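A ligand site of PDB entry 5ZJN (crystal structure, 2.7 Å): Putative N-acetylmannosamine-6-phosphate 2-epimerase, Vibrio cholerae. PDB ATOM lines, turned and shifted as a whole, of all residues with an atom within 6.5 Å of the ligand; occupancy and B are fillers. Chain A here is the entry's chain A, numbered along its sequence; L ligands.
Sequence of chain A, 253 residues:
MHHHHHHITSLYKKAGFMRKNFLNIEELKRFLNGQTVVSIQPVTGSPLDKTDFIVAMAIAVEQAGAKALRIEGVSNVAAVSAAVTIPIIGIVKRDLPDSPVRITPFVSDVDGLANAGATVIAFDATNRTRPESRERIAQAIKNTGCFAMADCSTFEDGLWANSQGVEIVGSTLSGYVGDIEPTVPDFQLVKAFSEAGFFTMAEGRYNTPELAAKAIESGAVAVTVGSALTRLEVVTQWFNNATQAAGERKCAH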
ATOM      1  N   SER A  39     -29.991  14.013  -1.176  1.00  0.00           N
ATOM      2  CA  SER A  39     -30.381  12.815  -0.454  1.00  0.00           C
ATOM      3  C   SER A  39     -29.602  12.754   0.870  1.00  0.00           C
ATOM      4  O   SER A  39     -28.373  12.622   0.875  1.00  0.00           O
ATOM      5  CB  SER A  39     -30.175  11.571  -1.322  1.00  0.00           C
ATOM      6  OG  SER A  39     -30.580  10.386  -0.663  1.00  0.00           O
ATOM      7  N   GLN A  41     -28.981  10.619   3.615  1.00  0.00           N
ATOM      8  CA  GLN A  41     -29.066   9.223   4.054  1.00  0.00           C
ATOM      9  C   GLN A  41     -27.708   8.779   4.537  1.00  0.00           C
ATOM     10  O   GLN A  41     -26.908   8.208   3.784  1.00  0.00           O
ATOM     11  CB  GLN A  41     -29.589   8.315   2.936  1.00  0.00           C
ATOM     12  CG  GLN A  41     -30.908   8.689   2.348  1.00  0.00           C
ATOM     13  CD  GLN A  41     -31.484   7.623   1.400  1.00  0.00           C
ATOM     14  OE1 GLN A  41     -31.098   6.452   1.443  1.00  0.00           O
ATOM     15  NE2 GLN A  41     -32.353   8.057   0.487  1.00  0.00           N
ATOM     16  N   ARG A  70     -34.401  14.234  -0.301  1.00  0.00           N
ATOM     17  CA  ARG A  70     -34.855  12.849  -0.180  1.00  0.00           C
ATOM     18  C   ARG A  70     -34.468  12.352   1.200  1.00  0.00           C
ATOM     19  O   ARG A  70     -33.280  12.348   1.558  1.00  0.00           O
ATOM     20  CB  ARG A  70     -34.277  11.946  -1.274  1.00  0.00           C
ATOM     21  CG  ARG A  70     -34.619  10.456  -1.072  1.00  0.00           C
ATOM     22  CD  ARG A  70     -33.956   9.553  -2.102  1.00  0.00           C
ATOM     23  NE  ARG A  70     -34.677   9.494  -3.358  1.00  0.00           N
ATOM     24  CZ  ARG A  70     -35.147   8.387  -3.904  1.00  0.00           C
ATOM     25  NH1 ARG A  70     -34.958   7.228  -3.304  1.00  0.00           N
ATOM     26  NH2 ARG A  70     -35.813   8.436  -5.058  1.00  0.00           N
ATOM     27  N   ILE A  91     -39.090   8.108   1.793  1.00  0.00           N
ATOM     28  CA  ILE A  91     -38.920   6.677   1.531  1.00  0.00           C
ATOM     29  C   ILE A  91     -38.744   5.937   2.849  1.00  0.00           C
ATOM     30  O   ILE A  91     -38.452   6.524   3.900  1.00  0.00           O
ATOM     31  CB  ILE A  91     -37.720   6.369   0.600  1.00  0.00           C
ATOM     32  CG1 ILE A  91     -36.416   6.930   1.174  1.00  0.00           C
ATOM     33  CG2 ILE A  91     -37.960   6.828  -0.842  1.00  0.00           C
ATOM     34  CD1 ILE A  91     -35.192   6.477   0.408  1.00  0.00           C
ATOM     35  N   LYS A  93     -36.608   2.363   3.523  1.00  0.00           N
ATOM     36  CA  LYS A  93     -35.775   1.346   2.894  1.00  0.00           C
ATOM     37  C   LYS A  93     -35.671   0.143   3.818  1.00  0.00           C
ATOM     38  O   LYS A  93     -35.256   0.266   4.974  1.00  0.00           O
ATOM     39  CB  LYS A  93     -34.397   1.936   2.565  1.00  0.00           C
ATOM     40  CG  LYS A  93     -33.381   0.918   2.137  1.00  0.00           C
ATOM     41  CD  LYS A  93     -32.061   1.590   1.758  1.00  0.00           C
ATOM     42  CE  LYS A  93     -32.258   2.758   0.806  1.00  0.00           C
ATOM     43  NZ  LYS A  93     -30.957   3.153   0.160  1.00  0.00           N
ATOM     44  N   ARG A 102     -36.333  -2.935  -1.964  1.00  0.00           N
ATOM     45  CA  ARG A 102     -35.967  -2.193  -0.762  1.00  0.00           C
ATOM     46  C   ARG A 102     -36.748  -0.906  -0.575  1.00  0.00           C
ATOM     47  O   ARG A 102     -37.155  -0.591   0.547  1.00  0.00           O
ATOM     48  CB  ARG A 102     -34.467  -1.824  -0.800  1.00  0.00           C
ATOM     49  CG  ARG A 102     -33.577  -2.991  -1.094  1.00  0.00           C
ATOM     50  CD  ARG A 102     -32.128  -2.569  -1.220  1.00  0.00           C
ATOM     51  NE  ARG A 102     -31.538  -2.323   0.094  1.00  0.00           N
ATOM     52  CZ  ARG A 102     -30.571  -1.436   0.332  1.00  0.00           C
ATOM     53  NH1 ARG A 102     -30.085  -0.698  -0.643  1.00  0.00           N
ATOM     54  NH2 ARG A 102     -30.110  -1.296   1.567  1.00  0.00           N
ATOM     55  N   ILE A 103     -37.020  -0.190  -1.655  1.00  0.00           N
ATOM     56  CA  ILE A 103     -37.519   1.184  -1.591  1.00  0.00           C
ATOM     57  C   ILE A 103     -39.035   1.134  -1.386  1.00  0.00           C
ATOM     58  O   ILE A 103     -39.782   0.795  -2.306  1.00  0.00           O
ATOM     59  CB  ILE A 103     -37.169   1.950  -2.865  1.00  0.00           C
ATOM     60  CG1 ILE A 103     -35.706   1.740  -3.241  1.00  0.00           C
ATOM     61  CG2 ILE A 103     -37.431   3.419  -2.676  1.00  0.00           C
ATOM     62  CD1 ILE A 103     -34.753   2.475  -2.403  1.00  0.00           C
ATOM     63  N   ASP A 151     -38.923   4.823  -8.730  1.00  0.00           N
ATOM     64  CA  ASP A 151     -37.510   4.470  -8.874  1.00  0.00           C
ATOM     65  C   ASP A 151     -37.402   3.252  -9.777  1.00  0.00           C
ATOM     66  O   ASP A 151     -37.824   2.153  -9.406  1.00  0.00           O
ATOM     67  CB  ASP A 151     -36.884   4.259  -7.490  1.00  0.00           C
ATOM     68  CG  ASP A 151     -36.728   5.577  -6.686  1.00  0.00           C
ATOM     69  OD1 ASP A 151     -36.483   6.652  -7.282  1.00  0.00           O
ATOM     70  OD2 ASP A 151     -36.865   5.531  -5.451  1.00  0.00           O
ATOM     71  N   THR A 172     -33.114   5.700 -10.403  1.00  0.00           N
ATOM     72  CA  THR A 172     -32.563   5.331  -9.098  1.00  0.00           C
ATOM     73  C   THR A 172     -32.029   3.880  -9.077  1.00  0.00           C
ATOM     74  O   THR A 172     -30.990   3.613  -8.473  1.00  0.00           O
ATOM     75  CB  THR A 172     -33.643   5.523  -8.046  1.00  0.00           C
ATOM     76  OG1 THR A 172     -34.180   6.849  -8.156  1.00  0.00           O
ATOM     77  CG2 THR A 172     -33.080   5.308  -6.673  1.00  0.00           C
ATOM     78  N   LEU A 173     -32.752   2.937  -9.699  1.00  0.00           N
ATOM     79  CA  LEU A 173     -32.455   1.505  -9.538  1.00  0.00           C
ATOM     80  C   LEU A 173     -31.691   0.913 -10.704  1.00  0.00           C
ATOM     81  O   LEU A 173     -31.484  -0.293 -10.753  1.00  0.00           O
ATOM     82  CB  LEU A 173     -33.735   0.720  -9.319  1.00  0.00           C
ATOM     83  CG  LEU A 173     -34.494   1.011  -8.020  1.00  0.00           C
ATOM     84  CD1 LEU A 173     -35.725   0.108  -7.938  1.00  0.00           C
ATOM     85  CD2 LEU A 173     -33.601   0.858  -6.777  1.00  0.00           C
ATOM     86  N   TYR A 176     -28.545  -1.705 -10.059  1.00  0.00           N
ATOM     87  CA  TYR A 176     -28.662  -2.277  -8.726  1.00  0.00           C
ATOM     88  C   TYR A 176     -29.573  -3.485  -8.684  1.00  0.00           C
ATOM     89  O   TYR A 176     -30.273  -3.716  -7.692  1.00  0.00           O
ATOM     90  CB  TYR A 176     -29.151  -1.224  -7.732  1.00  0.00           C
ATOM     91  CG  TYR A 176     -28.222  -0.047  -7.649  1.00  0.00           C
ATOM     92  CD1 TYR A 176     -27.019  -0.171  -6.972  1.00  0.00           C
ATOM     93  CD2 TYR A 176     -28.515   1.163  -8.261  1.00  0.00           C
ATOM     94  CE1 TYR A 176     -26.139   0.885  -6.881  1.00  0.00           C
ATOM     95  CE2 TYR A 176     -27.636   2.225  -8.185  1.00  0.00           C
ATOM     96  CZ  TYR A 176     -26.443   2.083  -7.490  1.00  0.00           C
ATOM     97  OH  TYR A 176     -25.523   3.112  -7.368  1.00  0.00           O
ATOM     98  N   GLU A 203     -30.948  10.024 -10.863  1.00  0.00           N
ATOM     99  CA  GLU A 203     -30.517   9.639  -9.526  1.00  0.00           C
ATOM    100  C   GLU A 203     -29.722   8.345  -9.624  1.00  0.00           C
ATOM    101  O   GLU A 203     -30.162   7.396 -10.276  1.00  0.00           O
ATOM    102  CB  GLU A 203     -31.710   9.469  -8.590  1.00  0.00           C
ATOM    103  CG  GLU A 203     -31.374   8.932  -7.204  1.00  0.00           C
ATOM    104  CD  GLU A 203     -32.534   9.068  -6.239  1.00  0.00           C
ATOM    105  OE1 GLU A 203     -33.481   9.826  -6.561  1.00  0.00           O
ATOM    106  OE2 GLU A 203     -32.540   8.374  -5.197  1.00  0.00           O
ATOM    107  N   GLY A 204     -28.572   8.315  -8.950  1.00  0.00           N
ATOM    108  CA  GLY A 204     -27.693   7.162  -8.914  1.00  0.00           C
ATOM    109  C   GLY A 204     -26.296   7.487  -9.407  1.00  0.00           C
ATOM    110  O   GLY A 204     -26.034   7.554 -10.609  1.00  0.00           O
ATOM    111  N   ARG A 205     -25.412   7.748  -8.439  1.00  0.00           N
ATOM    112  CA  ARG A 205     -23.963   7.837  -8.599  1.00  0.00           C
ATOM    113  C   ARG A 205     -23.516   9.022  -9.466  1.00  0.00           C
ATOM    114  O   ARG A 205     -22.447   8.979 -10.102  1.00  0.00           O
ATOM    115  CB  ARG A 205     -23.372   6.489  -9.025  1.00  0.00           C
ATOM    116  CG  ARG A 205     -23.494   5.994 -10.397  1.00  0.00           C
ATOM    117  CD  ARG A 205     -23.079   4.528 -10.387  1.00  0.00           C
ATOM    118  NE  ARG A 205     -24.217   3.625 -10.292  1.00  0.00           N
ATOM    119  CZ  ARG A 205     -24.958   3.236 -11.337  1.00  0.00           C
ATOM    120  NH1 ARG A 205     -24.669   3.682 -12.551  1.00  0.00           N
ATOM    121  NH2 ARG A 205     -25.975   2.405 -11.170  1.00  0.00           N
ATOM    122  N   TYR A 206     -24.327  10.081  -9.513  1.00  0.00           N
ATOM    123  CA  TYR A 206     -23.923  11.372 -10.073  1.00  0.00           C
ATOM    124  C   TYR A 206     -23.080  12.086  -9.014  1.00  0.00           C
ATOM    125  O   TYR A 206     -23.548  12.909  -8.214  1.00  0.00           O
ATOM    126  CB  TYR A 206     -25.140  12.200 -10.503  1.00  0.00           C
ATOM    127  CG  TYR A 206     -25.907  11.623 -11.660  1.00  0.00           C
ATOM    128  CD1 TYR A 206     -25.460  11.792 -12.975  1.00  0.00           C
ATOM    129  CD2 TYR A 206     -27.101  10.920 -11.468  1.00  0.00           C
ATOM    130  CE1 TYR A 206     -26.185  11.248 -14.072  1.00  0.00           C
ATOM    131  CE2 TYR A 206     -27.837  10.399 -12.549  1.00  0.00           C
ATOM    132  CZ  TYR A 206     -27.358  10.548 -13.843  1.00  0.00           C
ATOM    133  OH  TYR A 206     -28.060  10.031 -14.886  1.00  0.00           O
ATOM    134  N   ASN A 207     -21.800  11.727  -8.990  1.00  0.00           N
ATOM    135  CA  ASN A 207     -20.926  11.981  -7.869  1.00  0.00           C
ATOM    136  C   ASN A 207     -20.142  13.294  -7.936  1.00  0.00           C
ATOM    137  O   ASN A 207     -19.502  13.652  -6.941  1.00  0.00           O
ATOM    138  CB  ASN A 207     -19.970  10.791  -7.703  1.00  0.00           C
ATOM    139  CG  ASN A 207     -20.691   9.524  -7.315  1.00  0.00           C
ATOM    140  OD1 ASN A 207     -21.706   9.574  -6.604  1.00  0.00           O
ATOM    141  ND2 ASN A 207     -20.192   8.391  -7.774  1.00  0.00           N
ATOM    142  N   THR A 224     -30.793  13.933  -8.302  1.00  0.00           N
ATOM    143  CA  THR A 224     -30.684  13.634  -6.877  1.00  0.00           C
ATOM    144  C   THR A 224     -29.288  13.089  -6.586  1.00  0.00           C
ATOM    145  O   THR A 224     -28.790  12.218  -7.307  1.00  0.00           O
ATOM    146  CB  THR A 224     -31.755  12.641  -6.422  1.00  0.00           C
ATOM    147  OG1 THR A 224     -33.040  13.226  -6.591  1.00  0.00           O
ATOM    148  CG2 THR A 224     -31.540  12.272  -4.937  1.00  0.00           C
ATOM    149  N   VAL A 225     -28.655  13.630  -5.560  1.00  0.00           N
ATOM    150  CA  VAL A 225     -27.299  13.248  -5.213  1.00  0.00           C
ATOM    151  C   VAL A 225     -27.227  12.981  -3.710  1.00  0.00           C
ATOM    152  O   VAL A 225     -27.740  13.774  -2.914  1.00  0.00           O
ATOM    153  CB  VAL A 225     -26.277  14.309  -5.651  1.00  0.00           C
ATOM    154  CG1 VAL A 225     -24.884  13.905  -5.203  1.00  0.00           C
ATOM    155  CG2 VAL A 225     -26.335  14.468  -7.179  1.00  0.00           C
ATOM    156  N   GLY A 226     -26.627  11.855  -3.343  1.00  0.00           N
ATOM    157  CA  GLY A 226     -26.519  11.455  -1.946  1.00  0.00           C
ATOM    158  C   GLY A 226     -25.107  11.202  -1.407  1.00  0.00           C
ATOM    159  O   GLY A 226     -24.615  11.935  -0.558  1.00  0.00           O
ATOM    160  N   SER A 227     -24.476  10.137  -1.902  1.00  0.00           N
ATOM    161  CA  SER A 227     -23.206   9.690  -1.365  1.00  0.00           C
ATOM    162  C   SER A 227     -22.161  10.801  -1.391  1.00  0.00           C
ATOM    163  O   SER A 227     -21.477  11.043  -0.389  1.00  0.00           O
ATOM    164  CB  SER A 227     -22.704   8.470  -2.146  1.00  0.00           C
ATOM    165  OG  SER A 227     -23.648   7.422  -2.070  1.00  0.00           O
ATOM    166  N   ALA A 228     -22.031  11.498  -2.519  1.00  0.00           N
ATOM    167  CA  ALA A 228     -21.036  12.545  -2.642  1.00  0.00           C
ATOM    168  C   ALA A 228     -21.296  13.723  -1.698  1.00  0.00           C
ATOM    169  O   ALA A 228     -20.426  14.605  -1.582  1.00  0.00           O
ATOM    170  CB  ALA A 228     -20.969  13.015  -4.102  1.00  0.00           C
ATOM    171  N   ARG A 231     -22.601  11.117   2.794  1.00  0.00           N
ATOM    172  CA  ARG A 231     -21.970   9.893   3.257  1.00  0.00           C
ATOM    173  C   ARG A 231     -20.465  10.143   3.377  1.00  0.00           C
ATOM    174  O   ARG A 231     -19.703   9.866   2.438  1.00  0.00           O
ATOM    175  CB  ARG A 231     -22.310   8.725   2.305  1.00  0.00           C
ATOM    176  CG  ARG A 231     -23.691   8.164   2.540  1.00  0.00           C
ATOM    177  CD  ARG A 231     -24.020   7.056   1.568  1.00  0.00           C
ATOM    178  NE  ARG A 231     -25.298   6.431   1.933  1.00  0.00           N
ATOM    179  CZ  ARG A 231     -26.119   5.838   1.058  1.00  0.00           C
ATOM    180  NH1 ARG A 231     -25.824   5.819  -0.225  1.00  0.00           N
ATOM    181  NH2 ARG A 231     -27.252   5.309   1.492  1.00  0.00           N
ATOM    182  N   TRP A 238     -13.149   7.330  -1.038  1.00  0.00           N
ATOM    183  CA  TRP A 238     -12.829   7.713  -2.409  1.00  0.00           C
ATOM    184  C   TRP A 238     -11.488   8.419  -2.483  1.00  0.00           C
ATOM    185  O   TRP A 238     -10.708   8.198  -3.419  1.00  0.00           O
ATOM    186  CB  TRP A 238     -13.916   8.629  -2.966  1.00  0.00           C
ATOM    187  CG  TRP A 238     -15.199   7.937  -3.320  1.00  0.00           C
ATOM    188  CD1 TRP A 238     -15.409   6.587  -3.423  1.00  0.00           C
ATOM    189  CD2 TRP A 238     -16.445   8.562  -3.611  1.00  0.00           C
ATOM    190  NE1 TRP A 238     -16.716   6.345  -3.756  1.00  0.00           N
ATOM    191  CE2 TRP A 238     -17.377   7.535  -3.895  1.00  0.00           C
ATOM    192  CE3 TRP A 238     -16.876   9.896  -3.679  1.00  0.00           C
ATOM    193  CZ2 TRP A 238     -18.702   7.793  -4.218  1.00  0.00           C
ATOM    194  CZ3 TRP A 238     -18.195  10.157  -3.996  1.00  0.00           C
ATOM    195  CH2 TRP A 238     -19.099   9.098  -4.262  1.00  0.00           C
HETATM  196  N1  LIG L   1     -30.192   4.111  -3.627  1.00  0.00           N
HETATM  197  P1  LIG L   1     -26.118   8.425  -4.768  1.00  0.00           P
HETATM  198  C1  LIG L   1     -32.119   5.607  -3.057  1.00  0.00           C
HETATM  199  O1  LIG L   1     -32.499   6.651  -2.628  1.00  0.00           O
HETATM  200  C2  LIG L   1     -30.785   4.956  -2.594  1.00  0.00           C
HETATM  201  C3  LIG L   1     -29.821   6.043  -2.082  1.00  0.00           C
HETATM  202  O2  LIG L   1     -29.045   5.513  -1.016  1.00  0.00           O
HETATM  203  C4  LIG L   1     -28.888   6.675  -3.112  1.00  0.00           C
HETATM  204  O3  LIG L   1     -27.903   7.451  -2.434  1.00  0.00           O
HETATM  205  C5  LIG L   1     -29.603   7.589  -4.107  1.00  0.00           C
HETATM  206  O4  LIG L   1     -30.107   6.797  -5.191  1.00  0.00           O
HETATM  207  C6  LIG L   1     -28.705   8.702  -4.622  1.00  0.00           C
HETATM  208  O5  LIG L   1     -27.582   8.132  -5.318  1.00  0.00           O
HETATM  209  C7  LIG L   1     -30.419   2.778  -3.736  1.00  0.00           C
HETATM  210  O6  LIG L   1     -31.187   2.184  -2.987  1.00  0.00           O
HETATM  211  C8  LIG L   1     -29.643   2.074  -4.810  1.00  0.00           C
HETATM  212  O7  LIG L   1     -25.096   7.644  -5.568  1.00  0.00           O
HETATM  213  O8  LIG L   1     -25.878   9.893  -5.067  1.00  0.00           O
HETATM  214  O9  LIG L   1     -26.066   8.087  -3.330  1.00  0.00           O
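An oxygen (O2) of the ligand lies within hydrogen-bond range of the side-chain amino group (NZ) of Lys 93 (3.3 Å).
An oxygen (O4) of the ligand sits at hydrogen-bond distance from the side-chain carboxylate (OE2) of Glu 203, at 2.9 Å.
An oxygen (O7) of the ligand lies within hydrogen-bond range of the backbone NH of Arg 205 (2.9 Å).
An oxygen (O9) of the ligand lies within hydrogen-bond range of the backbone NH of Ser 227.
The side-chain amide oxygen (OE1) of Gln 41 lies within hydrogen-bond range of an oxygen (O2) of the ligand.
An oxygen (O9) of the ligand is in salt-bridge range of the guanidinium group of Arg 231, at 3.9 Å.
The side-chain hydroxyl (OG) of Ser 227 is in hydrogen-bond range of an oxygen (O9) of the ligand (2.8 Å).
An oxygen (O8) of the ligand sits at hydrogen-bond distance from the backbone NH (N) of Gly 226 (2.7 Å).
The guanidinium group (NH1) of Arg 70 lies within hydrogen-bond range of an oxygen (O1) of the ligand, at 2.6 Å.
The side-chain carboxylate of Asp 151 is in salt-bridge range of the guanidinium group of Arg 70, at 2.9 Å.
The guanidinium group (NE) of Arg 231 is in hydrogen-bond range of the backbone carbonyl oxygen (O) of Gln 41 (3.0 Å).
NE2 of Gln 41 is in hydrogen-bond range of OG of Ser 39 (3.1 Å).
The backbone carbonyl oxygen (O) of Val 225 is in hydrogen-bond range of the backbone NH (N) of Ser 39.
The side-chain hydroxyl (OG1) of Thr 172 is in hydrogen-bond range of the side-chain carboxylate (OD1) of Asp 151.
OH of Tyr 176 is in hydrogen-bond range of NE of Arg 205.
OE1 of Glu 203 lies close to OG1 of Thr 224 (3.4 Å).
The backbone carbonyl oxygen of Arg 205 sits at hydrogen-bond distance from the side-chain amide nitrogen of Asn 207 (3.3 Å).
NH1 of Arg 102 touches O6 of the ligand, at 3.9 Å.
Ile 103 touches the ligand (CD1 to O6, 3.6 Å).
Thr 172 touches the ligand (CG2 to O4, 3.6 Å).
CD2 of Tyr 176 touches C8 of the ligand, 3.7 Å away.
CA of Gly 204 touches O5 of the ligand (3.7 Å).
Val 225 touches the ligand (C to O8, 3.6 Å).
Hydrophobic or aromatic side chains within 4 Å of the ligand: Ile 103 and Tyr 176.
Within 4 Å of the ligand: Gln 41, Arg 70, Lys 93, Arg 102, Ile 103, Thr 172, Tyr 176, Glu 203, Gly 204, Arg 205, Val 225, Gly 226, Ser 227 and Arg 231.
Along chain A the residues within 4 Å of the ligand span positions 41 to 231.
The nearest printed residue that does not touch the ligand is Asn 207 (4.04 Å).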
